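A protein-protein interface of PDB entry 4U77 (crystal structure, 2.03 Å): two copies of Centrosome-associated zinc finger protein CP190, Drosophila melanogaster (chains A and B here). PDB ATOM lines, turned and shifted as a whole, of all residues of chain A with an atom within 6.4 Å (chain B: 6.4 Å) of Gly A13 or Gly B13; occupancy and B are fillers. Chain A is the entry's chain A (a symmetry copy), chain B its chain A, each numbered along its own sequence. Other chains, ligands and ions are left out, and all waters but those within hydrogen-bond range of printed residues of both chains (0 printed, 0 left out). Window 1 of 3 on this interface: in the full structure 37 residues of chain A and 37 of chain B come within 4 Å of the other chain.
Trp A12 touches Leu B17. Thr B90 touches Trp A12. O of Gly B13 touches CA of Gly A13, at 3.6 Å. N of Gly A13 touches CD2 of Leu B17, at 3.7 Å. Phe A16 touches Phe B16 (CE2 to CE2, 3.95 Å). Leu A17 touches Trp B12. Leu A17 touches Gly B13. CD1 of Trp B12 touches C of Thr A90, 3.5 Å away.
Gly A13 touches two residues of chain B. Of chain A, only Gly A13 (3.6 Å) and Leu A17 (3.7 Å) come within 4 Å of Gly B13. Printed residues of chain B within 4 Å of Thr A90: Trp B12 (3.5 Å). Printed residues of chain A within 4 Å of Trp B12: Leu A17 (3.8 Å) and Thr A90 (3.5 Å). Of the printed residues of chain B, Phe A16 touches Phe B16 (3.95 Å). Of the printed residues of chain B, Trp A12 touches Leu B17 and Thr B90. Printed residues of chain A within 4 Å of Leu B17: Trp A12 (3.8 Å) and Gly A13 (3.7 Å). Asp A10 touches none of the printed residues of chain B. The nearest residue of chain A that does not touch Gly B13 is Val A14 (4.2 Å). The nearest printed residue of chain B that does not touch Phe A16 is Leu B17 (4.4 Å).
Printed residues of chain A that touch a printed residue of chain B: Trp A12, Gly A13, Phe A16, Leu A17 and Thr A90. Hydrophobic or aromatic side chains of chain A within 4 Å of the printed part of chain B: Trp A12, Phe A16 and Leu A17. Along chain A the printed residues that touch a printed residue of chain B span positions 12 to 90. Printed residues of chain B that touch a printed residue of chain A: Trp B12, Gly B13, Phe B16, Leu B17 and Thr B90. Among the printed residues, no Asp or Glu carboxylate lies within 4 Å of a Lys or Arg side-chain nitrogen of the other chain.
Trp A12 touches Leu B17, and with the chains exchanged Leu A17 touches Trp B12. Trp A12 touches Thr B90, and with the chains exchanged Thr A90 touches Trp B12. Gly A13 touches Leu B17, and with the chains exchanged Leu A17 touches Gly B13. Phe B16 touches its own counterpart, Phe A16.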
ATOM      1  N   ASP A  10     -20.770 -21.857  -7.013  1.00  0.00           N
ATOM      2  CA  ASP A  10     -22.187 -22.135  -6.833  1.00  0.00           C
ATOM      3  C   ASP A  10     -22.738 -21.408  -5.610  1.00  0.00           C
ATOM      4  O   ASP A  10     -21.988 -21.057  -4.691  1.00  0.00           O
ATOM      5  CB  ASP A  10     -22.430 -23.643  -6.714  1.00  0.00           C
ATOM      6  CG  ASP A  10     -22.438 -24.339  -8.062  1.00  0.00           C
ATOM      7  OD1 ASP A  10     -23.161 -23.867  -8.968  1.00  0.00           O
ATOM      8  OD2 ASP A  10     -21.728 -25.355  -8.217  1.00  0.00           O
ATOM      9  N   ASN A  11     -24.051 -21.181  -5.623  1.00  0.00           N
ATOM     10  CA  ASN A  11     -24.752 -20.509  -4.531  1.00  0.00           C
ATOM     11  C   ASN A  11     -24.099 -19.188  -4.117  1.00  0.00           C
ATOM     12  O   ASN A  11     -23.872 -18.931  -2.932  1.00  0.00           O
ATOM     13  CB  ASN A  11     -24.854 -21.445  -3.322  1.00  0.00           C
ATOM     14  CG  ASN A  11     -25.454 -22.793  -3.680  1.00  0.00           C
ATOM     15  OD1 ASN A  11     -26.357 -22.885  -4.514  1.00  0.00           O
ATOM     16  ND2 ASN A  11     -24.952 -23.850  -3.054  1.00  0.00           N
ATOM     17  N   TRP A  12     -23.803 -18.352  -5.104  1.00  0.00           N
ATOM     18  CA  TRP A  12     -23.152 -17.073  -4.849  1.00  0.00           C
ATOM     19  C   TRP A  12     -24.014 -16.133  -4.005  1.00  0.00           C
ATOM     20  O   TRP A  12     -23.495 -15.394  -3.160  1.00  0.00           O
ATOM     21  CB  TRP A  12     -22.794 -16.401  -6.171  1.00  0.00           C
ATOM     22  CG  TRP A  12     -21.937 -15.202  -6.012  1.00  0.00           C
ATOM     23  CD1 TRP A  12     -22.276 -13.894  -6.278  1.00  0.00           C
ATOM     24  CD2 TRP A  12     -20.589 -15.180  -5.546  1.00  0.00           C
ATOM     25  NE1 TRP A  12     -21.202 -13.065  -6.011  1.00  0.00           N
ATOM     26  CE2 TRP A  12     -20.157 -13.833  -5.562  1.00  0.00           C
ATOM     27  CE3 TRP A  12     -19.691 -16.172  -5.137  1.00  0.00           C
ATOM     28  CZ2 TRP A  12     -18.878 -13.457  -5.174  1.00  0.00           C
ATOM     29  CZ3 TRP A  12     -18.425 -15.794  -4.757  1.00  0.00           C
ATOM     30  CH2 TRP A  12     -18.027 -14.449  -4.780  1.00  0.00           C
ATOM     31  N   GLY A  13     -25.323 -16.161  -4.243  1.00  0.00           N
ATOM     32  CA  GLY A  13     -26.257 -15.354  -3.474  1.00  0.00           C
ATOM     33  C   GLY A  13     -26.159 -15.658  -1.990  1.00  0.00           C
ATOM     34  O   GLY A  13     -26.121 -14.750  -1.158  1.00  0.00           O
ATOM     35  N   VAL A  14     -26.129 -16.946  -1.662  1.00  0.00           N
ATOM     36  CA  VAL A  14     -25.921 -17.385  -0.291  1.00  0.00           C
ATOM     37  C   VAL A  14     -24.614 -16.803   0.260  1.00  0.00           C
ATOM     38  O   VAL A  14     -24.610 -16.141   1.299  1.00  0.00           O
ATOM     39  CB  VAL A  14     -25.901 -18.932  -0.193  1.00  0.00           C
ATOM     40  CG1 VAL A  14     -25.424 -19.378   1.175  1.00  0.00           C
ATOM     41  CG2 VAL A  14     -27.284 -19.506  -0.488  1.00  0.00           C
ATOM     42  N   PHE A  15     -23.516 -17.029  -0.458  1.00  0.00           N
ATOM     43  CA  PHE A  15     -22.211 -16.520  -0.046  1.00  0.00           C
ATOM     44  C   PHE A  15     -22.239 -15.006   0.150  1.00  0.00           C
ATOM     45  O   PHE A  15     -21.827 -14.506   1.191  1.00  0.00           O
ATOM     46  CB  PHE A  15     -21.140 -16.899  -1.075  1.00  0.00           C
ATOM     47  CG  PHE A  15     -19.823 -16.188  -0.885  1.00  0.00           C
ATOM     48  CD1 PHE A  15     -18.911 -16.623   0.071  1.00  0.00           C
ATOM     49  CD2 PHE A  15     -19.481 -15.099  -1.680  1.00  0.00           C
ATOM     50  CE1 PHE A  15     -17.695 -15.975   0.240  1.00  0.00           C
ATOM     51  CE2 PHE A  15     -18.268 -14.448  -1.512  1.00  0.00           C
ATOM     52  CZ  PHE A  15     -17.374 -14.888  -0.557  1.00  0.00           C
ATOM     53  N   PHE A  16     -22.739 -14.282  -0.848  1.00  0.00           N
ATOM     54  CA  PHE A  16     -22.718 -12.828  -0.791  1.00  0.00           C
ATOM     55  C   PHE A  16     -23.578 -12.314   0.345  1.00  0.00           C
ATOM     56  O   PHE A  16     -23.196 -11.374   1.041  1.00  0.00           O
ATOM     57  CB  PHE A  16     -23.188 -12.212  -2.111  1.00  0.00           C
ATOM     58  CG  PHE A  16     -23.048 -10.720  -2.143  1.00  0.00           C
ATOM     59  CD1 PHE A  16     -21.820 -10.134  -2.392  1.00  0.00           C
ATOM     60  CD2 PHE A  16     -24.134  -9.904  -1.870  1.00  0.00           C
ATOM     61  CE1 PHE A  16     -21.677  -8.764  -2.394  1.00  0.00           C
ATOM     62  CE2 PHE A  16     -23.998  -8.530  -1.870  1.00  0.00           C
ATOM     63  CZ  PHE A  16     -22.768  -7.960  -2.129  1.00  0.00           C
ATOM     64  N   LEU A  17     -24.743 -12.936   0.515  1.00  0.00           N
ATOM     65  CA  LEU A  17     -25.683 -12.555   1.552  1.00  0.00           C
ATOM     66  C   LEU A  17     -25.016 -12.566   2.919  1.00  0.00           C
ATOM     67  O   LEU A  17     -25.102 -11.596   3.671  1.00  0.00           O
ATOM     68  CB  LEU A  17     -26.886 -13.495   1.557  1.00  0.00           C
ATOM     69  CG  LEU A  17     -28.186 -12.925   2.113  1.00  0.00           C
ATOM     70  CD1 LEU A  17     -28.573 -11.670   1.333  1.00  0.00           C
ATOM     71  CD2 LEU A  17     -29.287 -13.971   2.060  1.00  0.00           C
ATOM     72  N   GLN A  18     -24.355 -13.677   3.229  1.00  0.00           N
ATOM     73  CA  GLN A  18     -23.698 -13.837   4.518  1.00  0.00           C
ATOM     74  C   GLN A  18     -22.735 -12.684   4.793  1.00  0.00           C
ATOM     75  O   GLN A  18     -22.711 -12.154   5.900  1.00  0.00           O
ATOM     76  CB  GLN A  18     -22.957 -15.175   4.582  1.00  0.00           C
ATOM     77  CG  GLN A  18     -22.154 -15.376   5.851  1.00  0.00           C
ATOM     78  CD  GLN A  18     -21.518 -16.746   5.913  1.00  0.00           C
ATOM     79  OE1 GLN A  18     -21.725 -17.574   5.027  1.00  0.00           O
ATOM     80  NE2 GLN A  18     -20.744 -16.996   6.967  1.00  0.00           N
ATOM     81  N   THR A  90     -32.100 -10.445   5.205  1.00  0.00           N
ATOM     82  CA  THR A  90     -32.109 -11.877   5.512  1.00  0.00           C
ATOM     83  C   THR A  90     -33.150 -12.681   4.742  1.00  0.00           C
ATOM     84  O   THR A  90     -33.000 -13.885   4.557  1.00  0.00           O
ATOM     85  CB  THR A  90     -32.351 -12.113   7.024  1.00  0.00           C
ATOM     86  OG1 THR A  90     -33.676 -11.692   7.364  1.00  0.00           O
ATOM     87  CG2 THR A  90     -31.347 -11.346   7.863  1.00  0.00           C
ATOM     88  N   ASP B  10     -37.925 -17.711   0.636  1.00  0.00           N
ATOM     89  CA  ASP B  10     -36.866 -18.656   0.316  1.00  0.00           C
ATOM     90  C   ASP B  10     -35.939 -18.099  -0.761  1.00  0.00           C
ATOM     91  O   ASP B  10     -36.331 -17.223  -1.541  1.00  0.00           O
ATOM     92  CB  ASP B  10     -37.456 -19.999  -0.126  1.00  0.00           C
ATOM     93  CG  ASP B  10     -37.901 -20.853   1.046  1.00  0.00           C
ATOM     94  OD1 ASP B  10     -37.094 -21.038   1.985  1.00  0.00           O
ATOM     95  OD2 ASP B  10     -39.051 -21.341   1.029  1.00  0.00           O
ATOM     96  N   ASN B  11     -34.710 -18.615  -0.780  1.00  0.00           N
ATOM     97  CA  ASN B  11     -33.696 -18.210  -1.751  1.00  0.00           C
ATOM     98  C   ASN B  11     -33.518 -16.693  -1.842  1.00  0.00           C
ATOM     99  O   ASN B  11     -33.502 -16.116  -2.932  1.00  0.00           O
ATOM    100  CB  ASN B  11     -34.035 -18.782  -3.130  1.00  0.00           C
ATOM    101  CG  ASN B  11     -34.267 -20.284  -3.096  1.00  0.00           C
ATOM    102  OD1 ASN B  11     -33.604 -21.011  -2.355  1.00  0.00           O
ATOM    103  ND2 ASN B  11     -35.216 -20.754  -3.896  1.00  0.00           N
ATOM    104  N   TRP B  12     -33.383 -16.053  -0.687  1.00  0.00           N
ATOM    105  CA  TRP B  12     -33.237 -14.604  -0.632  1.00  0.00           C
ATOM    106  C   TRP B  12     -31.957 -14.117  -1.315  1.00  0.00           C
ATOM    107  O   TRP B  12     -31.951 -13.059  -1.956  1.00  0.00           O
ATOM    108  CB  TRP B  12     -33.262 -14.135   0.819  1.00  0.00           C
ATOM    109  CG  TRP B  12     -33.337 -12.662   0.964  1.00  0.00           C
ATOM    110  CD1 TRP B  12     -32.371 -11.823   1.473  1.00  0.00           C
ATOM    111  CD2 TRP B  12     -34.436 -11.830   0.594  1.00  0.00           C
ATOM    112  NE1 TRP B  12     -32.820 -10.516   1.449  1.00  0.00           N
ATOM    113  CE2 TRP B  12     -34.084 -10.497   0.915  1.00  0.00           C
ATOM    114  CE3 TRP B  12     -35.697 -12.083   0.045  1.00  0.00           C
ATOM    115  CZ2 TRP B  12     -34.941  -9.428   0.691  1.00  0.00           C
ATOM    116  CZ3 TRP B  12     -36.543 -11.019  -0.172  1.00  0.00           C
ATOM    117  CH2 TRP B  12     -36.163  -9.707   0.153  1.00  0.00           C
ATOM    118  N   GLY B  13     -30.882 -14.886  -1.167  1.00  0.00           N
ATOM    119  CA  GLY B  13     -29.617 -14.562  -1.807  1.00  0.00           C
ATOM    120  C   GLY B  13     -29.771 -14.452  -3.313  1.00  0.00           C
ATOM    121  O   GLY B  13     -29.270 -13.514  -3.936  1.00  0.00           O
ATOM    122  N   VAL B  14     -30.463 -15.426  -3.898  1.00  0.00           N
ATOM    123  CA  VAL B  14     -30.789 -15.391  -5.315  1.00  0.00           C
ATOM    124  C   VAL B  14     -31.549 -14.104  -5.654  1.00  0.00           C
ATOM    125  O   VAL B  14     -31.137 -13.343  -6.531  1.00  0.00           O
ATOM    126  CB  VAL B  14     -31.623 -16.630  -5.729  1.00  0.00           C
ATOM    127  CG1 VAL B  14     -32.181 -16.459  -7.129  1.00  0.00           C
ATOM    128  CG2 VAL B  14     -30.779 -17.899  -5.644  1.00  0.00           C
ATOM    129  N   PHE B  15     -32.641 -13.854  -4.933  1.00  0.00           N
ATOM    130  CA  PHE B  15     -33.447 -12.656  -5.151  1.00  0.00           C
ATOM    131  C   PHE B  15     -32.604 -11.387  -5.031  1.00  0.00           C
ATOM    132  O   PHE B  15     -32.624 -10.543  -5.919  1.00  0.00           O
ATOM    133  CB  PHE B  15     -34.615 -12.610  -4.161  1.00  0.00           C
ATOM    134  CG  PHE B  15     -35.337 -11.285  -4.119  1.00  0.00           C
ATOM    135  CD1 PHE B  15     -36.281 -10.960  -5.087  1.00  0.00           C
ATOM    136  CD2 PHE B  15     -35.094 -10.374  -3.097  1.00  0.00           C
ATOM    137  CE1 PHE B  15     -36.952  -9.746  -5.045  1.00  0.00           C
ATOM    138  CE2 PHE B  15     -35.762  -9.160  -3.053  1.00  0.00           C
ATOM    139  CZ  PHE B  15     -36.693  -8.848  -4.023  1.00  0.00           C
ATOM    140  N   PHE B  16     -31.858 -11.265  -3.937  1.00  0.00           N
ATOM    141  CA  PHE B  16     -31.099 -10.049  -3.691  1.00  0.00           C
ATOM    142  C   PHE B  16     -30.030  -9.850  -4.746  1.00  0.00           C
ATOM    143  O   PHE B  16     -29.809  -8.731  -5.208  1.00  0.00           O
ATOM    144  CB  PHE B  16     -30.454 -10.067  -2.303  1.00  0.00           C
ATOM    145  CG  PHE B  16     -29.779  -8.774  -1.955  1.00  0.00           C
ATOM    146  CD1 PHE B  16     -30.520  -7.690  -1.516  1.00  0.00           C
ATOM    147  CD2 PHE B  16     -28.412  -8.626  -2.118  1.00  0.00           C
ATOM    148  CE1 PHE B  16     -29.911  -6.490  -1.222  1.00  0.00           C
ATOM    149  CE2 PHE B  16     -27.795  -7.425  -1.826  1.00  0.00           C
ATOM    150  CZ  PHE B  16     -28.545  -6.356  -1.380  1.00  0.00           C
ATOM    151  N   LEU B  17     -29.367 -10.945  -5.111  1.00  0.00           N
ATOM    152  CA  LEU B  17     -28.307 -10.918  -6.101  1.00  0.00           C
ATOM    153  C   LEU B  17     -28.795 -10.290  -7.398  1.00  0.00           C
ATOM    154  O   LEU B  17     -28.160  -9.384  -7.937  1.00  0.00           O
ATOM    155  CB  LEU B  17     -27.792 -12.331  -6.374  1.00  0.00           C
ATOM    156  CG  LEU B  17     -26.357 -12.439  -6.877  1.00  0.00           C
ATOM    157  CD1 LEU B  17     -25.410 -11.776  -5.880  1.00  0.00           C
ATOM    158  CD2 LEU B  17     -25.988 -13.895  -7.109  1.00  0.00           C
ATOM    159  N   GLN B  18     -29.925 -10.786  -7.891  1.00  0.00           N
ATOM    160  CA  GLN B  18     -30.487 -10.301  -9.143  1.00  0.00           C
ATOM    161  C   GLN B  18     -30.670  -8.786  -9.115  1.00  0.00           C
ATOM    162  O   GLN B  18     -30.340  -8.108 -10.085  1.00  0.00           O
ATOM    163  CB  GLN B  18     -31.820 -10.992  -9.437  1.00  0.00           C
ATOM    164  CG  GLN B  18     -32.529 -10.467 -10.670  1.00  0.00           C
ATOM    165  CD  GLN B  18     -33.791 -11.240 -10.975  1.00  0.00           C
ATOM    166  OE1 GLN B  18     -34.112 -12.214 -10.294  1.00  0.00           O
ATOM    167  NE2 GLN B  18     -34.515 -10.815 -12.009  1.00  0.00           N
ATOM    168  N   THR B  90     -21.545 -11.848  -9.621  1.00  0.00           N
ATOM    169  CA  THR B  90     -22.281 -12.964 -10.217  1.00  0.00           C
ATOM    170  C   THR B  90     -21.877 -14.338  -9.694  1.00  0.00           C
ATOM    171  O   THR B  90     -22.656 -15.284  -9.753  1.00  0.00           O
ATOM    172  CB  THR B  90     -22.112 -12.974 -11.757  1.00  0.00           C
ATOM    173  OG1 THR B  90     -20.748 -13.262 -12.082  1.00  0.00           O
ATOM    174  CG2 THR B  90     -22.500 -11.636 -12.357  1.00  0.00           C
